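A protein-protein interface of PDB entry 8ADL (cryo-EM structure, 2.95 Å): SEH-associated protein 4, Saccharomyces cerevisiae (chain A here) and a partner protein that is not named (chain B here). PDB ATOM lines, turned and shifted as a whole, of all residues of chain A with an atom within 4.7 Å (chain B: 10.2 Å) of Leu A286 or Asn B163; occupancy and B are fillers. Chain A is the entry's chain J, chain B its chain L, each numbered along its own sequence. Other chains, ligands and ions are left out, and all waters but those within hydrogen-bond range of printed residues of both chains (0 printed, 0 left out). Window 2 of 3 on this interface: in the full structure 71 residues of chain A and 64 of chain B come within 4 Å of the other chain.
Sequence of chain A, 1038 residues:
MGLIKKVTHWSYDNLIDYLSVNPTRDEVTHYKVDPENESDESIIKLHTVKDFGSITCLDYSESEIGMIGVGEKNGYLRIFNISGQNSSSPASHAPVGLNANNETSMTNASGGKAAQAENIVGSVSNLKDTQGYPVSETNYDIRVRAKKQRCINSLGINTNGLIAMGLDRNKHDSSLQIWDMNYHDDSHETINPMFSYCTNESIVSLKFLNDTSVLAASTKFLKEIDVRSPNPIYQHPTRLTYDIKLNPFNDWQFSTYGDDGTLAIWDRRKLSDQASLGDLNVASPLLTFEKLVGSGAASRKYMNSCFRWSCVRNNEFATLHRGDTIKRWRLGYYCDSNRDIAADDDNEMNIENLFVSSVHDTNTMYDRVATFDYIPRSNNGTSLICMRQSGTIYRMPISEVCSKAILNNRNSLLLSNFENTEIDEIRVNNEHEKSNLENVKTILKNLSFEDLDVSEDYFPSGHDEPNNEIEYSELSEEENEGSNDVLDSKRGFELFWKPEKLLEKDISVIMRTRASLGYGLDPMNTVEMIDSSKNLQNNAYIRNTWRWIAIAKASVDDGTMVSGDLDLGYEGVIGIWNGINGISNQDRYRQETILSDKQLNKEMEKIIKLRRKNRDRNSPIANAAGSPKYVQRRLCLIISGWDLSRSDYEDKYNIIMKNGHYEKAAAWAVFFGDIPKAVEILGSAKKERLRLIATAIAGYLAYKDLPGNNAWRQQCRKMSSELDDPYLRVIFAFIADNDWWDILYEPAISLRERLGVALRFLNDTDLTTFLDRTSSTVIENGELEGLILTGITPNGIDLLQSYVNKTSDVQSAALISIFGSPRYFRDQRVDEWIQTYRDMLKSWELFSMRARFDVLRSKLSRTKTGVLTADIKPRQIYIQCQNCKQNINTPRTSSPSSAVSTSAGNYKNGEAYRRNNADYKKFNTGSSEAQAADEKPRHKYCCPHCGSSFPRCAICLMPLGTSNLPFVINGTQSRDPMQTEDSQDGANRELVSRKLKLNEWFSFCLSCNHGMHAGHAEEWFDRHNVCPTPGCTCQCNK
O of Leu A286 touches ND2 of Asn B163, 3.8 Å away. ND2 of Asn B163 touches CD2 of Leu A287, at 3.8 Å. His B164 touches Thr A288. CZ of Phe A355 touches CG of Tyr B77 (3.4 Å). CE1 of Phe A355 touches OG of Ser B110, 3.5 Å away. Phe A355 touches Tyr B112. Phe A355 touches Asn B163 (CB to OD1, 3.3 Å). CG2 of Val A356 touches O of His B164, 3.4 Å away. O of Val A356 touches O of Leu B165 (3.97 Å). Gln B166 touches Val A356.
Of the 15 printed residues of chain B, 7 touch a printed residue of chain A. Hydrophobic or aromatic side chains of chain B that line the printed part of chain A: Tyr B77, Tyr B112 and His B164. Along chain B the printed residues that touch a printed residue of chain A span positions 77 to 166. Printed residues of chain A that touch a printed residue of chain B: Leu A286, Leu A287, Thr A288, Leu A354, Phe A355 and Val A356. Hydrophobic or aromatic side chains of chain A within 4 Å of the printed part of chain B: Leu A287, Phe A355 and Val A356.
The side-chain hydroxyl (OG) of Ser B110 is in hydrogen-bond range of the backbone carbonyl oxygen (O) of Tyr B77 (3.0 Å). The backbone NH of Ser B110 lies within hydrogen-bond range of the side-chain amide oxygen of Asn B130, 2.5 Å away. OG of Ser B167 lies within hydrogen-bond range of OH of Tyr B112. The backbone carbonyl oxygen (O) of Ile A265 sits at hydrogen-bond distance from the backbone NH (N) of Leu A286, 2.9 Å away. The backbone carbonyl oxygen (O) of Ile A265 is in hydrogen-bond range of the backbone NH (N) of Leu A287 (3.1 Å).
The side-chain amide oxygen (OD1) of Asn B163 sits close to the backbone carbonyl oxygen (O) of Leu A354 (2.9 Å). The backbone carbonyl oxygen (O) of Asn B163 lies within hydrogen-bond range of the backbone NH (N) of Val A356, 3.4 Å away.
Leu A286 touches just one residue of chain B: Asn B163. Of chain A, only Leu A286 (3.8 Å), Leu A287 (3.8 Å), Leu A354 (2.9 Å), Phe A355 (3.3 Å) and Val A356 (3.4 Å) come within 4 Å of Asn B163. Printed residues of chain B within 4 Å of Leu A287: Asn B163 (3.8 Å). Of chain B, only Asn B163 comes within 4 Å of Leu A354. Printed residues of chain B within 4 Å of Phe A355: Tyr B77, Ser B110, Tyr B112 and Asn B163. Of the printed residues of chain A, Tyr B112 touches Phe A355. Of the printed residues of chain A, His B164 touches Thr A288 (3.2 Å) and Val A356 (3.4 Å). Asn B130 touches none of the printed residues of chain A. Asn A353 touches none of the printed residues of chain B. The nearest printed residue of chain A that does not touch Asn B163 is Asn A353 (5.9 Å).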
ATOM      1  N   GLN A 253     -19.840  -3.827  16.451  1.00  0.00           N
ATOM      2  CA  GLN A 253     -20.994  -4.030  15.587  1.00  0.00           C
ATOM      3  C   GLN A 253     -22.073  -3.010  15.921  1.00  0.00           C
ATOM      4  O   GLN A 253     -22.503  -2.911  17.075  1.00  0.00           O
ATOM      5  CB  GLN A 253     -21.542  -5.449  15.729  1.00  0.00           C
ATOM      6  CG  GLN A 253     -20.717  -6.503  15.022  1.00  0.00           C
ATOM      7  CD  GLN A 253     -21.142  -7.905  15.389  1.00  0.00           C
ATOM      8  OE1 GLN A 253     -22.182  -8.105  16.015  1.00  0.00           O
ATOM      9  NE2 GLN A 253     -20.339  -8.887  15.001  1.00  0.00           N
ATOM     10  N   ILE A 265     -26.582  -4.299   9.335  1.00  0.00           N
ATOM     11  CA  ILE A 265     -25.670  -4.462  10.461  1.00  0.00           C
ATOM     12  C   ILE A 265     -24.250  -4.249   9.957  1.00  0.00           C
ATOM     13  O   ILE A 265     -23.835  -4.871   8.972  1.00  0.00           O
ATOM     14  CB  ILE A 265     -25.829  -5.848  11.105  1.00  0.00           C
ATOM     15  CG1 ILE A 265     -27.273  -6.058  11.557  1.00  0.00           C
ATOM     16  CG2 ILE A 265     -24.870  -6.015  12.272  1.00  0.00           C
ATOM     17  CD1 ILE A 265     -27.517  -7.412  12.154  1.00  0.00           C
ATOM     18  N   TRP A 266     -23.509  -3.363  10.613  1.00  0.00           N
ATOM     19  CA  TRP A 266     -22.172  -3.000  10.171  1.00  0.00           C
ATOM     20  C   TRP A 266     -21.120  -3.525  11.138  1.00  0.00           C
ATOM     21  O   TRP A 266     -21.423  -4.049  12.213  1.00  0.00           O
ATOM     22  CB  TRP A 266     -22.028  -1.480  10.042  1.00  0.00           C
ATOM     23  CG  TRP A 266     -23.048  -0.808   9.185  1.00  0.00           C
ATOM     24  CD1 TRP A 266     -24.321  -0.474   9.533  1.00  0.00           C
ATOM     25  CD2 TRP A 266     -22.867  -0.361   7.839  1.00  0.00           C
ATOM     26  NE1 TRP A 266     -24.951   0.144   8.482  1.00  0.00           N
ATOM     27  CE2 TRP A 266     -24.079   0.225   7.429  1.00  0.00           C
ATOM     28  CE3 TRP A 266     -21.801  -0.406   6.939  1.00  0.00           C
ATOM     29  CZ2 TRP A 266     -24.253   0.762   6.159  1.00  0.00           C
ATOM     30  CZ3 TRP A 266     -21.974   0.126   5.682  1.00  0.00           C
ATOM     31  CH2 TRP A 266     -23.191   0.705   5.301  1.00  0.00           C
ATOM     32  N   ASP A 267     -19.863  -3.370  10.729  1.00  0.00           N
ATOM     33  CA  ASP A 267     -18.708  -3.563  11.593  1.00  0.00           C
ATOM     34  C   ASP A 267     -17.784  -2.367  11.428  1.00  0.00           C
ATOM     35  O   ASP A 267     -17.498  -1.953  10.301  1.00  0.00           O
ATOM     36  CB  ASP A 267     -17.969  -4.861  11.259  1.00  0.00           C
ATOM     37  CG  ASP A 267     -17.284  -5.466  12.466  1.00  0.00           C
ATOM     38  OD1 ASP A 267     -16.703  -4.704  13.265  1.00  0.00           O
ATOM     39  OD2 ASP A 267     -17.327  -6.705  12.617  1.00  0.00           O
ATOM     40  N   LYS A 270     -14.447  -3.102   9.595  1.00  0.00           N
ATOM     41  CA  LYS A 270     -14.562  -3.205   8.143  1.00  0.00           C
ATOM     42  C   LYS A 270     -14.578  -1.825   7.494  1.00  0.00           C
ATOM     43  O   LYS A 270     -13.991  -1.629   6.423  1.00  0.00           O
ATOM     44  CB  LYS A 270     -15.819  -3.987   7.767  1.00  0.00           C
ATOM     45  CG  LYS A 270     -15.759  -4.626   6.391  1.00  0.00           C
ATOM     46  CD  LYS A 270     -16.752  -5.768   6.265  1.00  0.00           C
ATOM     47  CE  LYS A 270     -16.289  -6.988   7.043  1.00  0.00           C
ATOM     48  NZ  LYS A 270     -14.984  -7.500   6.543  1.00  0.00           N
ATOM     49  N   SER A 284     -18.225  -3.056   2.626  1.00  0.00           N
ATOM     50  CA  SER A 284     -19.613  -3.469   2.527  1.00  0.00           C
ATOM     51  C   SER A 284     -20.229  -3.616   3.914  1.00  0.00           C
ATOM     52  O   SER A 284     -19.514  -3.795   4.904  1.00  0.00           O
ATOM     53  CB  SER A 284     -19.706  -4.787   1.763  1.00  0.00           C
ATOM     54  OG  SER A 284     -18.912  -5.789   2.375  1.00  0.00           O
ATOM     55  N   PRO A 285     -21.556  -3.518   4.022  1.00  0.00           N
ATOM     56  CA  PRO A 285     -22.214  -3.871   5.283  1.00  0.00           C
ATOM     57  C   PRO A 285     -22.046  -5.350   5.584  1.00  0.00           C
ATOM     58  O   PRO A 285     -21.927  -6.183   4.683  1.00  0.00           O
ATOM     59  CB  PRO A 285     -23.685  -3.520   5.035  1.00  0.00           C
ATOM     60  CG  PRO A 285     -23.673  -2.566   3.905  1.00  0.00           C
ATOM     61  CD  PRO A 285     -22.500  -2.929   3.055  1.00  0.00           C
ATOM     62  N   LEU A 286     -22.030  -5.670   6.879  1.00  0.00           N
ATOM     63  CA  LEU A 286     -21.835  -7.058   7.280  1.00  0.00           C
ATOM     64  C   LEU A 286     -23.073  -7.896   6.993  1.00  0.00           C
ATOM     65  O   LEU A 286     -22.954  -9.076   6.647  1.00  0.00           O
ATOM     66  CB  LEU A 286     -21.456  -7.114   8.760  1.00  0.00           C
ATOM     67  CG  LEU A 286     -20.756  -8.360   9.288  1.00  0.00           C
ATOM     68  CD1 LEU A 286     -19.453  -8.572   8.546  1.00  0.00           C
ATOM     69  CD2 LEU A 286     -20.487  -8.196  10.765  1.00  0.00           C
ATOM     70  N   LEU A 287     -24.261  -7.305   7.115  1.00  0.00           N
ATOM     71  CA  LEU A 287     -25.497  -7.894   6.620  1.00  0.00           C
ATOM     72  C   LEU A 287     -26.364  -6.787   6.043  1.00  0.00           C
ATOM     73  O   LEU A 287     -26.180  -5.606   6.347  1.00  0.00           O
ATOM     74  CB  LEU A 287     -26.273  -8.641   7.715  1.00  0.00           C
ATOM     75  CG  LEU A 287     -25.709  -9.953   8.257  1.00  0.00           C
ATOM     76  CD1 LEU A 287     -26.560 -10.458   9.401  1.00  0.00           C
ATOM     77  CD2 LEU A 287     -25.650 -10.983   7.150  1.00  0.00           C
ATOM     78  N   THR A 288     -27.314  -7.178   5.198  1.00  0.00           N
ATOM     79  CA  THR A 288     -28.294  -6.239   4.672  1.00  0.00           C
ATOM     80  C   THR A 288     -29.622  -6.955   4.467  1.00  0.00           C
ATOM     81  O   THR A 288     -29.661  -8.091   3.989  1.00  0.00           O
ATOM     82  CB  THR A 288     -27.799  -5.570   3.375  1.00  0.00           C
ATOM     83  OG1 THR A 288     -28.800  -4.676   2.876  1.00  0.00           O
ATOM     84  CG2 THR A 288     -27.410  -6.592   2.304  1.00  0.00           C
ATOM     85  N   GLU A 352     -15.807 -11.155  12.299  1.00  0.00           N
ATOM     86  CA  GLU A 352     -16.716 -12.273  12.091  1.00  0.00           C
ATOM     87  C   GLU A 352     -17.713 -11.943  10.988  1.00  0.00           C
ATOM     88  O   GLU A 352     -18.402 -10.920  11.051  1.00  0.00           O
ATOM     89  CB  GLU A 352     -17.456 -12.612  13.383  1.00  0.00           C
ATOM     90  CG  GLU A 352     -16.590 -12.560  14.625  1.00  0.00           C
ATOM     91  CD  GLU A 352     -17.357 -12.925  15.877  1.00  0.00           C
ATOM     92  OE1 GLU A 352     -18.601 -13.006  15.809  1.00  0.00           O
ATOM     93  OE2 GLU A 352     -16.717 -13.135  16.928  1.00  0.00           O
ATOM     94  N   ASN A 353     -17.785 -12.809   9.981  1.00  0.00           N
ATOM     95  CA  ASN A 353     -18.745 -12.655   8.898  1.00  0.00           C
ATOM     96  C   ASN A 353     -20.066 -13.285   9.322  1.00  0.00           C
ATOM     97  O   ASN A 353     -20.114 -14.471   9.660  1.00  0.00           O
ATOM     98  CB  ASN A 353     -18.226 -13.306   7.617  1.00  0.00           C
ATOM     99  CG  ASN A 353     -16.882 -12.757   7.189  1.00  0.00           C
ATOM    100  OD1 ASN A 353     -16.452 -11.704   7.657  1.00  0.00           O
ATOM    101  ND2 ASN A 353     -16.212 -13.467   6.290  1.00  0.00           N
ATOM    102  N   LEU A 354     -21.130 -12.490   9.305  1.00  0.00           N
ATOM    103  CA  LEU A 354     -22.412 -12.909   9.848  1.00  0.00           C
ATOM    104  C   LEU A 354     -23.306 -13.499   8.766  1.00  0.00           C
ATOM    105  O   LEU A 354     -23.183 -13.174   7.583  1.00  0.00           O
ATOM    106  CB  LEU A 354     -23.128 -11.739  10.525  1.00  0.00           C
ATOM    107  CG  LEU A 354     -22.492 -11.166  11.791  1.00  0.00           C
ATOM    108  CD1 LEU A 354     -23.341 -10.039  12.346  1.00  0.00           C
ATOM    109  CD2 LEU A 354     -22.300 -12.249  12.833  1.00  0.00           C
ATOM    110  N   PHE A 355     -24.206 -14.382   9.191  1.00  0.00           N
ATOM    111  CA  PHE A 355     -25.267 -14.902   8.342  1.00  0.00           C
ATOM    112  C   PHE A 355     -26.436 -15.301   9.230  1.00  0.00           C
ATOM    113  O   PHE A 355     -26.270 -15.571  10.422  1.00  0.00           O
ATOM    114  CB  PHE A 355     -24.793 -16.080   7.480  1.00  0.00           C
ATOM    115  CG  PHE A 355     -24.466 -17.321   8.258  1.00  0.00           C
ATOM    116  CD1 PHE A 355     -23.236 -17.462   8.879  1.00  0.00           C
ATOM    117  CD2 PHE A 355     -25.377 -18.363   8.342  1.00  0.00           C
ATOM    118  CE1 PHE A 355     -22.931 -18.603   9.586  1.00  0.00           C
ATOM    119  CE2 PHE A 355     -25.077 -19.504   9.050  1.00  0.00           C
ATOM    120  CZ  PHE A 355     -23.854 -19.624   9.670  1.00  0.00           C
ATOM    121  N   VAL A 356     -27.623 -15.337   8.635  1.00  0.00           N
ATOM    122  CA  VAL A 356     -28.846 -15.624   9.378  1.00  0.00           C
ATOM    123  C   VAL A 356     -28.999 -17.131   9.527  1.00  0.00           C
ATOM    124  O   VAL A 356     -29.037 -17.863   8.532  1.00  0.00           O
ATOM    125  CB  VAL A 356     -30.069 -15.011   8.684  1.00  0.00           C
ATOM    126  CG1 VAL A 356     -31.333 -15.361   9.443  1.00  0.00           C
ATOM    127  CG2 VAL A 356     -29.910 -13.510   8.572  1.00  0.00           C
ATOM    128  N   TYR B  77     -20.332 -23.676  12.545  1.00  0.00           N
ATOM    129  CA  TYR B  77     -20.450 -22.652  11.520  1.00  0.00           C
ATOM    130  C   TYR B  77     -19.104 -22.172  10.996  1.00  0.00           C
ATOM    131  O   TYR B  77     -19.078 -21.388  10.044  1.00  0.00           O
ATOM    132  CB  TYR B  77     -21.244 -21.462  12.061  1.00  0.00           C
ATOM    133  CG  TYR B  77     -22.736 -21.699  12.118  1.00  0.00           C
ATOM    134  CD1 TYR B  77     -23.329 -22.704  11.365  1.00  0.00           C
ATOM    135  CD2 TYR B  77     -23.553 -20.908  12.914  1.00  0.00           C
ATOM    136  CE1 TYR B  77     -24.692 -22.920  11.413  1.00  0.00           C
ATOM    137  CE2 TYR B  77     -24.917 -21.117  12.968  1.00  0.00           C
ATOM    138  CZ  TYR B  77     -25.480 -22.122  12.213  1.00  0.00           C
ATOM    139  OH  TYR B  77     -26.836 -22.336  12.263  1.00  0.00           O
ATOM    140  N   LYS B  79     -17.089 -23.908   9.287  1.00  0.00           N
ATOM    141  CA  LYS B  79     -16.811 -24.692   8.078  1.00  0.00           C
ATOM    142  C   LYS B  79     -15.868 -25.867   8.342  1.00  0.00           C
ATOM    143  O   LYS B  79     -15.042 -26.219   7.499  1.00  0.00           O
ATOM    144  CB  LYS B  79     -16.264 -23.808   6.952  1.00  0.00           C
ATOM    145  CG  LYS B  79     -17.045 -22.523   6.720  1.00  0.00           C
ATOM    146  CD  LYS B  79     -16.156 -21.424   6.174  1.00  0.00           C
ATOM    147  CE  LYS B  79     -16.934 -20.504   5.251  1.00  0.00           C
ATOM    148  NZ  LYS B  79     -16.049 -19.521   4.570  1.00  0.00           N
ATOM    149  N   GLY B 109     -18.346 -23.681   3.320  1.00  0.00           N
ATOM    150  CA  GLY B 109     -19.620 -23.195   3.806  1.00  0.00           C
ATOM    151  C   GLY B 109     -19.922 -23.689   5.204  1.00  0.00           C
ATOM    152  O   GLY B 109     -19.425 -24.744   5.611  1.00  0.00           O
ATOM    153  N   SER B 110     -20.718 -22.929   5.952  1.00  0.00           N
ATOM    154  CA  SER B 110     -21.000 -23.262   7.343  1.00  0.00           C
ATOM    155  C   SER B 110     -21.888 -24.497   7.403  1.00  0.00           C
ATOM    156  O   SER B 110     -22.998 -24.499   6.865  1.00  0.00           O
ATOM    157  CB  SER B 110     -21.672 -22.082   8.037  1.00  0.00           C
ATOM    158  OG  SER B 110     -20.947 -20.885   7.815  1.00  0.00           O
ATOM    159  N   TYR B 112     -24.293 -27.564   8.628  1.00  0.00           N
ATOM    160  CA  TYR B 112     -25.546 -27.588   9.374  1.00  0.00           C
ATOM    161  C   TYR B 112     -25.862 -28.935   9.999  1.00  0.00           C
ATOM    162  O   TYR B 112     -26.395 -28.977  11.108  1.00  0.00           O
ATOM    163  CB  TYR B 112     -26.712 -27.176   8.468  1.00  0.00           C
ATOM    164  CG  TYR B 112     -26.920 -25.683   8.376  1.00  0.00           C
ATOM    165  CD1 TYR B 112     -26.061 -24.888   7.633  1.00  0.00           C
ATOM    166  CD2 TYR B 112     -27.972 -25.068   9.040  1.00  0.00           C
ATOM    167  CE1 TYR B 112     -26.245 -23.523   7.548  1.00  0.00           C
ATOM    168  CE2 TYR B 112     -28.165 -23.703   8.960  1.00  0.00           C
ATOM    169  CZ  TYR B 112     -27.298 -22.937   8.213  1.00  0.00           C
ATOM    170  OH  TYR B 112     -27.486 -21.577   8.128  1.00  0.00           O
ATOM    171  N   ASN B 130     -24.258 -24.615   4.074  1.00  0.00           N
ATOM    172  CA  ASN B 130     -24.888 -23.577   3.257  1.00  0.00           C
ATOM    173  C   ASN B 130     -24.089 -23.309   1.982  1.00  0.00           C
ATOM    174  O   ASN B 130     -23.775 -22.172   1.633  1.00  0.00           O
ATOM    175  CB  ASN B 130     -25.072 -22.302   4.072  1.00  0.00           C
ATOM    176  CG  ASN B 130     -23.790 -21.834   4.728  1.00  0.00           C
ATOM    177  OD1 ASN B 130     -22.762 -22.500   4.653  1.00  0.00           O
ATOM    178  ND2 ASN B 130     -23.848 -20.677   5.376  1.00  0.00           N
ATOM    179  N   ILE B 159     -26.929 -23.211  -6.448  1.00  0.00           N
ATOM    180  CA  ILE B 159     -26.125 -22.098  -5.955  1.00  0.00           C
ATOM    181  C   ILE B 159     -26.264 -22.050  -4.438  1.00  0.00           C
ATOM    182  O   ILE B 159     -27.290 -22.498  -3.905  1.00  0.00           O
ATOM    183  CB  ILE B 159     -26.548 -20.775  -6.612  1.00  0.00           C
ATOM    184  CG1 ILE B 159     -28.072 -20.683  -6.692  1.00  0.00           C
ATOM    185  CG2 ILE B 159     -25.931 -20.647  -7.994  1.00  0.00           C
ATOM    186  CD1 ILE B 159     -28.579 -19.320  -7.108  1.00  0.00           C
ATOM    187  N   PRO B 160     -25.261 -21.555  -3.705  1.00  0.00           N
ATOM    188  CA  PRO B 160     -25.413 -21.425  -2.258  1.00  0.00           C
ATOM    189  C   PRO B 160     -26.464 -20.389  -1.909  1.00  0.00           C
ATOM    190  O   PRO B 160     -26.696 -19.437  -2.674  1.00  0.00           O
ATOM    191  CB  PRO B 160     -24.014 -20.980  -1.794  1.00  0.00           C
ATOM    192  CG  PRO B 160     -23.097 -21.395  -2.885  1.00  0.00           C
ATOM    193  CD  PRO B 160     -23.886 -21.259  -4.144  1.00  0.00           C
ATOM    194  N   PRO B 161     -27.145 -20.544  -0.773  1.00  0.00           N
ATOM    195  CA  PRO B 161     -28.126 -19.539  -0.351  1.00  0.00           C
ATOM    196  C   PRO B 161     -27.456 -18.223   0.013  1.00  0.00           C
ATOM    197  O   PRO B 161     -26.270 -18.166   0.348  1.00  0.00           O
ATOM    198  CB  PRO B 161     -28.793 -20.177   0.871  1.00  0.00           C
ATOM    199  CG  PRO B 161     -27.812 -21.184   1.357  1.00  0.00           C
ATOM    200  CD  PRO B 161     -27.113 -21.700   0.138  1.00  0.00           C
ATOM    201  N   ALA B 162     -28.240 -17.151  -0.074  1.00  0.00           N
ATOM    202  CA  ALA B 162     -27.722 -15.813   0.157  1.00  0.00           C
ATOM    203  C   ALA B 162     -27.365 -15.609   1.629  1.00  0.00           C
ATOM    204  O   ALA B 162     -27.707 -16.409   2.505  1.00  0.00           O
ATOM    205  CB  ALA B 162     -28.737 -14.762  -0.292  1.00  0.00           C
ATOM    206  N   ASN B 163     -26.657 -14.507   1.884  1.00  0.00           N
ATOM    207  CA  ASN B 163     -26.133 -14.226   3.218  1.00  0.00           C
ATOM    208  C   ASN B 163     -27.248 -13.921   4.213  1.00  0.00           C
ATOM    209  O   ASN B 163     -27.170 -14.318   5.381  1.00  0.00           O
ATOM    210  CB  ASN B 163     -25.146 -13.062   3.148  1.00  0.00           C
ATOM    211  CG  ASN B 163     -24.111 -13.112   4.247  1.00  0.00           C
ATOM    212  OD1 ASN B 163     -24.007 -14.100   4.970  1.00  0.00           O
ATOM    213  ND2 ASN B 163     -23.339 -12.041   4.381  1.00  0.00           N
ATOM    214  N   HIS B 164     -28.292 -13.223   3.768  1.00  0.00           N
ATOM    215  CA  HIS B 164     -29.326 -12.705   4.653  1.00  0.00           C
ATOM    216  C   HIS B 164     -30.553 -13.597   4.755  1.00  0.00           C
ATOM    217  O   HIS B 164     -31.434 -13.314   5.573  1.00  0.00           O
ATOM    218  CB  HIS B 164     -29.764 -11.321   4.174  1.00  0.00           C
ATOM    219  CG  HIS B 164     -30.015 -11.252   2.701  1.00  0.00           C
ATOM    220  ND1 HIS B 164     -29.015 -11.002   1.786  1.00  0.00           N
ATOM    221  CD2 HIS B 164     -31.151 -11.408   1.982  1.00  0.00           C
ATOM    222  CE1 HIS B 164     -29.525 -11.008   0.567  1.00  0.00           C
ATOM    223  NE2 HIS B 164     -30.819 -11.250   0.659  1.00  0.00           N
ATOM    224  N   LEU B 165     -30.642 -14.649   3.952  1.00  0.00           N
ATOM    225  CA  LEU B 165     -31.787 -15.544   3.990  1.00  0.00           C
ATOM    226  C   LEU B 165     -31.467 -16.723   4.894  1.00  0.00           C
ATOM    227  O   LEU B 165     -30.364 -17.273   4.841  1.00  0.00           O
ATOM    228  CB  LEU B 165     -32.138 -16.042   2.588  1.00  0.00           C
ATOM    229  CG  LEU B 165     -32.550 -15.000   1.552  1.00  0.00           C
ATOM    230  CD1 LEU B 165     -32.677 -15.643   0.184  1.00  0.00           C
ATOM    231  CD2 LEU B 165     -33.853 -14.334   1.953  1.00  0.00           C
ATOM    232  N   GLN B 166     -32.426 -17.106   5.731  1.00  0.00           N
ATOM    233  CA  GLN B 166     -32.200 -18.266   6.575  1.00  0.00           C
ATOM    234  C   GLN B 166     -32.294 -19.541   5.748  1.00  0.00           C
ATOM    235  O   GLN B 166     -32.955 -19.592   4.708  1.00  0.00           O
ATOM    236  CB  GLN B 166     -33.191 -18.315   7.738  1.00  0.00           C
ATOM    237  CG  GLN B 166     -34.632 -18.510   7.340  1.00  0.00           C
ATOM    238  CD  GLN B 166     -35.535 -18.711   8.538  1.00  0.00           C
ATOM    239  OE1 GLN B 166     -35.068 -18.808   9.671  1.00  0.00           O
ATOM    240  NE2 GLN B 166     -36.837 -18.771   8.293  1.00  0.00           N
ATOM    241  N   SER B 167     -31.612 -20.576   6.224  1.00  0.00           N
ATOM    242  CA  SER B 167     -31.553 -21.850   5.532  1.00  0.00           C
ATOM    243  C   SER B 167     -31.443 -22.953   6.568  1.00  0.00           C
ATOM    244  O   SER B 167     -30.931 -22.738   7.669  1.00  0.00           O
ATOM    245  CB  SER B 167     -30.371 -21.904   4.559  1.00  0.00           C
ATOM    246  OG  SER B 167     -29.151 -21.638   5.226  1.00  0.00           O
